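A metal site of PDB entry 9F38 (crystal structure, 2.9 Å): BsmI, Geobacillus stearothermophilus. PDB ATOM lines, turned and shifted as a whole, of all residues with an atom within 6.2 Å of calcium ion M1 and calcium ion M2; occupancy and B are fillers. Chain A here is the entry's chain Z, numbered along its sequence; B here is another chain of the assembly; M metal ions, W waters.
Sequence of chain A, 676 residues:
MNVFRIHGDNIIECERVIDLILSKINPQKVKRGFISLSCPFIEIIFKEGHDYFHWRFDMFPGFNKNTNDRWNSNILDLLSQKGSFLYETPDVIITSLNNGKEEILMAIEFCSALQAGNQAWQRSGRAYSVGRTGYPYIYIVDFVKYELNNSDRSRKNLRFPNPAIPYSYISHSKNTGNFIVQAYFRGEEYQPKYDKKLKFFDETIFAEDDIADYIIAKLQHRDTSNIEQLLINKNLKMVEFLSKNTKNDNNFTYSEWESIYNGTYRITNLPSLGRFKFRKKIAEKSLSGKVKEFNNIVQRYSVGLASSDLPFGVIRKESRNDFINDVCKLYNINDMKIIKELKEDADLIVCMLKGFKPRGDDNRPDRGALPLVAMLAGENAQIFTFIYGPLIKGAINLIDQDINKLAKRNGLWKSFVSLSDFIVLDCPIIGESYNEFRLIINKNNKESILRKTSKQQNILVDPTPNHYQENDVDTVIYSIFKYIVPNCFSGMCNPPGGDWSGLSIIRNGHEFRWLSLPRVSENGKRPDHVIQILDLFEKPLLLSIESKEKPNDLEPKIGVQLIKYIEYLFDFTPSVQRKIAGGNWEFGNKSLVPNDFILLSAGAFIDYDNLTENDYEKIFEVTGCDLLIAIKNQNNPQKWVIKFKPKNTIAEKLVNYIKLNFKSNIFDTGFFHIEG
Calcium ion M1 is bound by O of Phe 110, OD2 of Asp 91, OP1 of DC 6 of chain B and OE2 of Glu 109.
Calcium ion M1 has four donor atoms within binding distance.
Slightly farther from calcium ion M1 lies OD1 of Asp 91 (3.1 Å).
Water W1 bridges OD1 of Asp 9 (2.6 Å) and O of Thr 89 (3.3 Å).
Calcium ion M2 is bound by OD2 of Asp 9 (2.1 Å).
OD1 of Asp 91 binds calcium ion M2, 2.2 Å away.
OP1 of DC 6 of chain B binds calcium ion M2, 2.8 Å away.
Calcium ion M2 is bound by O3' of DG 5 of chain B (2.8 Å).
Slightly farther from calcium ion M2 lies water W1 (2.9 Å).
OE2 of Glu 109 lies close to NH2 of Arg 123 (3.6 Å).
The side-chain carboxylate (OD2) of Asp 499 lies within salt-bridge range of the guanidinium group (NH2) of Arg 16, at 3.2 Å.
The guanidinium group of Arg 123 lies within salt-bridge range of OP2 of DA 7 of chain B.
OP2 of DG 5 of chain B lies within salt-bridge range of NH2 of Arg 126 (3.2 Å).
OE1 of Glu 109 is in salt-bridge range of NH1 of Arg 126 (3.5 Å).
OP2 of DC 6 of chain B lies within salt-bridge range of NH1 of Arg 126 (2.7 Å).
OP2 of DC 6 of chain B lies within salt-bridge range of the guanidinium group (NH2) of Arg 123.
The side-chain sulfur (SG) of Cys 111 lies close to the guanidinium group (NH2) of Arg 123 (3.7 Å).
Within 4 Å of calcium ion M2: Asp 9, Asp 91, DG 5 of chain B and DC 6 of chain B.
The nearest printed residue that does not touch calcium ion M2 is Gly 497 (4.03 Å).
Merely in contact with calcium ion M1: Arg 123 and Asp 499.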
ATOM      1  N   ASP A   9      12.212 -17.613  14.259  1.00  0.00           N
ATOM      2  CA  ASP A   9      13.209 -18.686  14.096  1.00  0.00           C
ATOM      3  C   ASP A   9      14.453 -18.359  14.931  1.00  0.00           C
ATOM      4  O   ASP A   9      15.029 -19.250  15.545  1.00  0.00           O
ATOM      5  CB  ASP A   9      13.654 -18.803  12.625  1.00  0.00           C
ATOM      6  CG  ASP A   9      12.587 -19.193  11.644  1.00  0.00           C
ATOM      7  OD1 ASP A   9      11.820 -20.120  11.933  1.00  0.00           O
ATOM      8  OD2 ASP A   9      12.540 -18.574  10.559  1.00  0.00           O
ATOM      9  N   GLU A  13      15.041 -12.641  12.972  1.00  0.00           N
ATOM     10  CA  GLU A  13      13.684 -12.656  12.432  1.00  0.00           C
ATOM     11  C   GLU A  13      12.754 -11.829  13.320  1.00  0.00           C
ATOM     12  O   GLU A  13      11.944 -11.073  12.813  1.00  0.00           O
ATOM     13  CB  GLU A  13      13.142 -14.090  12.294  1.00  0.00           C
ATOM     14  CG  GLU A  13      14.127 -15.103  11.706  1.00  0.00           C
ATOM     15  CD  GLU A  13      14.354 -15.076  10.212  1.00  0.00           C
ATOM     16  OE1 GLU A  13      13.392 -14.788   9.457  1.00  0.00           O
ATOM     17  OE2 GLU A  13      15.494 -15.373   9.777  1.00  0.00           O
ATOM     18  N   ARG A  16      13.312  -8.084  12.855  1.00  0.00           N
ATOM     19  CA  ARG A  16      12.811  -7.552  11.593  1.00  0.00           C
ATOM     20  C   ARG A  16      11.387  -7.025  11.727  1.00  0.00           C
ATOM     21  O   ARG A  16      11.050  -6.002  11.135  1.00  0.00           O
ATOM     22  CB  ARG A  16      12.962  -8.575  10.457  1.00  0.00           C
ATOM     23  CG  ARG A  16      14.413  -8.765  10.050  1.00  0.00           C
ATOM     24  CD  ARG A  16      14.568  -8.984   8.557  1.00  0.00           C
ATOM     25  NE  ARG A  16      14.273 -10.360   8.154  1.00  0.00           N
ATOM     26  CZ  ARG A  16      15.192 -11.248   7.785  1.00  0.00           C
ATOM     27  NH1 ARG A  16      16.482 -10.913   7.751  1.00  0.00           N
ATOM     28  NH2 ARG A  16      14.837 -12.477   7.452  1.00  0.00           N
ATOM     29  N   THR A  89       6.754 -24.067   8.898  1.00  0.00           N
ATOM     30  CA  THR A  89       6.931 -23.045   9.896  1.00  0.00           C
ATOM     31  C   THR A  89       7.208 -21.670   9.331  1.00  0.00           C
ATOM     32  O   THR A  89       8.198 -21.476   8.611  1.00  0.00           O
ATOM     33  CB  THR A  89       8.039 -23.499  10.838  1.00  0.00           C
ATOM     34  OG1 THR A  89       7.661 -24.747  11.419  1.00  0.00           O
ATOM     35  CG2 THR A  89       8.314 -22.512  11.923  1.00  0.00           C
ATOM     36  N   PRO A  90       6.356 -20.663   9.653  1.00  0.00           N
ATOM     37  CA  PRO A  90       6.637 -19.296   9.191  1.00  0.00           C
ATOM     38  C   PRO A  90       7.835 -18.693   9.932  1.00  0.00           C
ATOM     39  O   PRO A  90       8.270 -19.241  10.944  1.00  0.00           O
ATOM     40  CB  PRO A  90       5.354 -18.550   9.510  1.00  0.00           C
ATOM     41  CG  PRO A  90       4.828 -19.248  10.705  1.00  0.00           C
ATOM     42  CD  PRO A  90       5.164 -20.709  10.515  1.00  0.00           C
ATOM     43  N   ASP A  91       8.361 -17.575   9.436  1.00  0.00           N
ATOM     44  CA  ASP A  91       9.523 -16.948  10.070  1.00  0.00           C
ATOM     45  C   ASP A  91       9.165 -16.322  11.412  1.00  0.00           C
ATOM     46  O   ASP A  91       9.943 -16.440  12.362  1.00  0.00           O
ATOM     47  CB  ASP A  91      10.218 -15.958   9.139  1.00  0.00           C
ATOM     48  CG  ASP A  91      10.942 -16.613   7.969  1.00  0.00           C
ATOM     49  OD1 ASP A  91      11.170 -17.847   8.013  1.00  0.00           O
ATOM     50  OD2 ASP A  91      11.280 -15.898   7.009  1.00  0.00           O
ATOM     51  N   GLU A 109       6.414 -14.365   6.813  1.00  0.00           N
ATOM     52  CA  GLU A 109       7.522 -15.081   6.206  1.00  0.00           C
ATOM     53  C   GLU A 109       8.333 -14.093   5.383  1.00  0.00           C
ATOM     54  O   GLU A 109       7.772 -13.327   4.607  1.00  0.00           O
ATOM     55  CB  GLU A 109       6.997 -16.217   5.325  1.00  0.00           C
ATOM     56  CG  GLU A 109       8.073 -16.950   4.563  1.00  0.00           C
ATOM     57  CD  GLU A 109       8.881 -17.930   5.384  1.00  0.00           C
ATOM     58  OE1 GLU A 109       8.357 -18.413   6.418  1.00  0.00           O
ATOM     59  OE2 GLU A 109      10.033 -18.219   4.998  1.00  0.00           O
ATOM     60  N   PHE A 110       9.649 -14.076   5.576  1.00  0.00           N
ATOM     61  CA  PHE A 110      10.571 -13.182   4.874  1.00  0.00           C
ATOM     62  C   PHE A 110      11.374 -13.993   3.853  1.00  0.00           C
ATOM     63  O   PHE A 110      12.038 -14.945   4.250  1.00  0.00           O
ATOM     64  CB  PHE A 110      11.562 -12.565   5.879  1.00  0.00           C
ATOM     65  CG  PHE A 110      10.956 -11.907   7.099  1.00  0.00           C
ATOM     66  CD1 PHE A 110      10.060 -10.872   6.966  1.00  0.00           C
ATOM     67  CD2 PHE A 110      11.310 -12.314   8.370  1.00  0.00           C
ATOM     68  CE1 PHE A 110       9.539 -10.245   8.084  1.00  0.00           C
ATOM     69  CE2 PHE A 110      10.791 -11.670   9.484  1.00  0.00           C
ATOM     70  CZ  PHE A 110       9.922 -10.648   9.333  1.00  0.00           C
ATOM     71  N   CYS A 111      11.333 -13.618   2.567  1.00  0.00           N
ATOM     72  CA  CYS A 111      12.081 -14.367   1.555  1.00  0.00           C
ATOM     73  C   CYS A 111      12.931 -13.490   0.655  1.00  0.00           C
ATOM     74  O   CYS A 111      12.422 -12.795  -0.208  1.00  0.00           O
ATOM     75  CB  CYS A 111      11.157 -15.262   0.732  1.00  0.00           C
ATOM     76  SG  CYS A 111      12.020 -16.565  -0.200  1.00  0.00           S
ATOM     77  N   SER A 112      14.239 -13.587   0.835  1.00  0.00           N
ATOM     78  CA  SER A 112      15.198 -12.876  -0.009  1.00  0.00           C
ATOM     79  C   SER A 112      15.575 -13.683  -1.240  1.00  0.00           C
ATOM     80  O   SER A 112      15.884 -13.101  -2.288  1.00  0.00           O
ATOM     81  CB  SER A 112      16.444 -12.538   0.795  1.00  0.00           C
ATOM     82  OG  SER A 112      16.363 -11.159   1.126  1.00  0.00           O
ATOM     83  N   ARG A 123       7.885 -22.442  -0.435  1.00  0.00           N
ATOM     84  CA  ARG A 123       7.225 -22.160   0.827  1.00  0.00           C
ATOM     85  C   ARG A 123       5.746 -21.787   0.654  1.00  0.00           C
ATOM     86  O   ARG A 123       5.209 -20.995   1.419  1.00  0.00           O
ATOM     87  CB  ARG A 123       7.977 -21.132   1.687  1.00  0.00           C
ATOM     88  CG  ARG A 123       8.720 -20.041   0.952  1.00  0.00           C
ATOM     89  CD  ARG A 123       9.845 -19.540   1.873  1.00  0.00           C
ATOM     90  NE  ARG A 123      11.045 -19.876   1.171  1.00  0.00           N
ATOM     91  CZ  ARG A 123      12.305 -19.594   1.437  1.00  0.00           C
ATOM     92  NH1 ARG A 123      13.268 -19.984   0.610  1.00  0.00           N
ATOM     93  NH2 ARG A 123      12.630 -18.929   2.540  1.00  0.00           N
ATOM     94  N   ARG A 126       3.328 -23.320   3.744  1.00  0.00           N
ATOM     95  CA  ARG A 126       2.978 -22.532   4.929  1.00  0.00           C
ATOM     96  C   ARG A 126       1.888 -21.556   4.614  1.00  0.00           C
ATOM     97  O   ARG A 126       0.994 -21.402   5.427  1.00  0.00           O
ATOM     98  CB  ARG A 126       4.184 -21.870   5.614  1.00  0.00           C
ATOM     99  CG  ARG A 126       5.165 -21.196   4.692  1.00  0.00           C
ATOM    100  CD  ARG A 126       6.497 -20.999   5.381  1.00  0.00           C
ATOM    101  NE  ARG A 126       7.213 -22.262   5.460  1.00  0.00           N
ATOM    102  CZ  ARG A 126       8.504 -22.430   5.156  1.00  0.00           C
ATOM    103  NH1 ARG A 126       9.249 -21.382   4.834  1.00  0.00           N
ATOM    104  NH2 ARG A 126       9.059 -23.631   5.215  1.00  0.00           N
ATOM    105  N   GLY A 497      18.949 -21.620  11.386  1.00  0.00           N
ATOM    106  CA  GLY A 497      17.682 -21.520  10.678  1.00  0.00           C
ATOM    107  C   GLY A 497      17.408 -20.139  10.126  1.00  0.00           C
ATOM    108  O   GLY A 497      16.256 -19.720  10.037  1.00  0.00           O
ATOM    109  N   GLY A 498      18.458 -19.437   9.740  1.00  0.00           N
ATOM    110  CA  GLY A 498      18.353 -18.083   9.237  1.00  0.00           C
ATOM    111  C   GLY A 498      18.483 -17.921   7.736  1.00  0.00           C
ATOM    112  O   GLY A 498      19.022 -18.786   7.052  1.00  0.00           O
ATOM    113  N   ASP A 499      18.007 -16.768   7.239  1.00  0.00           N
ATOM    114  CA  ASP A 499      18.024 -16.379   5.827  1.00  0.00           C
ATOM    115  C   ASP A 499      19.443 -16.089   5.312  1.00  0.00           C
ATOM    116  O   ASP A 499      20.379 -15.966   6.088  1.00  0.00           O
ATOM    117  CB  ASP A 499      17.146 -15.116   5.633  1.00  0.00           C
ATOM    118  CG  ASP A 499      15.654 -15.331   5.757  1.00  0.00           C
ATOM    119  OD1 ASP A 499      15.241 -16.167   6.584  1.00  0.00           O
ATOM    120  OD2 ASP A 499      14.896 -14.632   5.038  1.00  0.00           O
ATOM    121  P    DG B   5       9.619 -26.232   6.892  1.00  0.00           P
ATOM    122  OP1  DG B   5       8.439 -25.772   7.654  1.00  0.00           O
ATOM    123  OP2  DG B   5       9.455 -26.825   5.542  1.00  0.00           O
ATOM    124  O5'  DG B   5      10.668 -25.027   6.775  1.00  0.00           O
ATOM    125  C5'  DG B   5      10.901 -24.150   7.876  1.00  0.00           C
ATOM    126  C4'  DG B   5      12.376 -23.806   8.014  1.00  0.00           C
ATOM    127  O4'  DG B   5      13.154 -25.027   8.128  1.00  0.00           O
ATOM    128  C3'  DG B   5      13.007 -23.087   6.836  1.00  0.00           C
ATOM    129  O3'  DG B   5      12.730 -21.683   6.872  1.00  0.00           O
ATOM    130  C2'  DG B   5      14.475 -23.354   7.110  1.00  0.00           C
ATOM    131  C1'  DG B   5      14.444 -24.801   7.582  1.00  0.00           C
ATOM    132  N9   DG B   5      14.702 -25.756   6.512  1.00  0.00           N
ATOM    133  C8   DG B   5      13.780 -26.466   5.780  1.00  0.00           C
ATOM    134  N7   DG B   5      14.324 -27.220   4.862  1.00  0.00           N
ATOM    135  C5   DG B   5      15.674 -26.911   4.935  1.00  0.00           C
ATOM    136  C6   DG B   5      16.764 -27.375   4.159  1.00  0.00           C
ATOM    137  O6   DG B   5      16.743 -28.188   3.225  1.00  0.00           O
ATOM    138  N1   DG B   5      17.962 -26.801   4.566  1.00  0.00           N
ATOM    139  C2   DG B   5      18.088 -25.873   5.570  1.00  0.00           C
ATOM    140  N2   DG B   5      19.323 -25.440   5.833  1.00  0.00           N
ATOM    141  N3   DG B   5      17.085 -25.450   6.311  1.00  0.00           N
ATOM    142  C4   DG B   5      15.910 -25.996   5.934  1.00  0.00           C
ATOM    143  P    DC B   6      12.748 -20.819   5.519  1.00  0.00           P
ATOM    144  OP1  DC B   6      12.359 -19.436   5.870  1.00  0.00           O
ATOM    145  OP2  DC B   6      11.969 -21.560   4.490  1.00  0.00           O
ATOM    146  O5'  DC B   6      14.281 -20.831   5.067  1.00  0.00           O
ATOM    147  C5'  DC B   6      15.290 -20.278   5.919  1.00  0.00           C
ATOM    148  C4'  DC B   6      16.687 -20.507   5.354  1.00  0.00           C
ATOM    149  O4'  DC B   6      16.995 -21.923   5.335  1.00  0.00           O
ATOM    150  C3'  DC B   6      16.873 -20.077   3.919  1.00  0.00           C
ATOM    151  O3'  DC B   6      17.083 -18.692   3.815  1.00  0.00           O
ATOM    152  C2'  DC B   6      18.112 -20.865   3.522  1.00  0.00           C
ATOM    153  C1'  DC B   6      17.874 -22.193   4.244  1.00  0.00           C
ATOM    154  N1   DC B   6      17.280 -23.247   3.353  1.00  0.00           N
ATOM    155  C2   DC B   6      18.094 -23.997   2.507  1.00  0.00           C
ATOM    156  O2   DC B   6      19.316 -23.817   2.549  1.00  0.00           O
ATOM    157  N3   DC B   6      17.532 -24.924   1.698  1.00  0.00           N
ATOM    158  C4   DC B   6      16.213 -25.085   1.695  1.00  0.00           C
ATOM    159  N4   DC B   6      15.690 -26.000   0.876  1.00  0.00           N
ATOM    160  C5   DC B   6      15.356 -24.322   2.517  1.00  0.00           C
ATOM    161  C6   DC B   6      15.923 -23.425   3.332  1.00  0.00           C
ATOM    162  P    DA B   7      16.737 -17.964   2.440  1.00  0.00           P
ATOM    163  OP1  DA B   7      16.503 -16.525   2.721  1.00  0.00           O
ATOM    164  OP2  DA B   7      15.689 -18.765   1.770  1.00  0.00           O
ATOM    165  O5'  DA B   7      18.111 -18.120   1.620  1.00  0.00           O
ATOM    166  C5'  DA B   7      18.086 -18.426   0.240  1.00  0.00           C
ATOM    167  C4'  DA B   7      19.229 -19.328  -0.133  1.00  0.00           C
ATOM    168  O4'  DA B   7      18.910 -20.688   0.226  1.00  0.00           O
ATOM    169  C3'  DA B   7      19.508 -19.352  -1.617  1.00  0.00           C
ATOM    170  O3'  DA B   7      20.500 -18.392  -1.884  1.00  0.00           O
ATOM    171  C2'  DA B   7      20.018 -20.768  -1.867  1.00  0.00           C
ATOM    172  C1'  DA B   7      19.402 -21.589  -0.740  1.00  0.00           C
ATOM    173  N9   DA B   7      18.301 -22.448  -1.151  1.00  0.00           N
ATOM    174  C8   DA B   7      16.999 -22.331  -0.786  1.00  0.00           C
ATOM    175  N7   DA B   7      16.226 -23.280  -1.251  1.00  0.00           N
ATOM    176  C5   DA B   7      17.103 -24.097  -1.953  1.00  0.00           C
ATOM    177  C6   DA B   7      16.904 -25.293  -2.662  1.00  0.00           C
ATOM    178  N6   DA B   7      15.719 -25.877  -2.799  1.00  0.00           N
ATOM    179  N1   DA B   7      17.982 -25.862  -3.235  1.00  0.00           N
ATOM    180  C2   DA B   7      19.169 -25.261  -3.101  1.00  0.00           C
ATOM    181  N3   DA B   7      19.483 -24.143  -2.448  1.00  0.00           N
ATOM    182  C4   DA B   7      18.383 -23.599  -1.891  1.00  0.00           C
HETATM  183 CA    CA M   1      12.319 -16.809   5.272  1.00  0.00          CA
HETATM  184 CA    CA M   2      12.456 -19.528   8.694  1.00  0.00          CA
HETATM  185  O   HOH W   1      11.178 -21.751  10.080  1.00  0.00           O
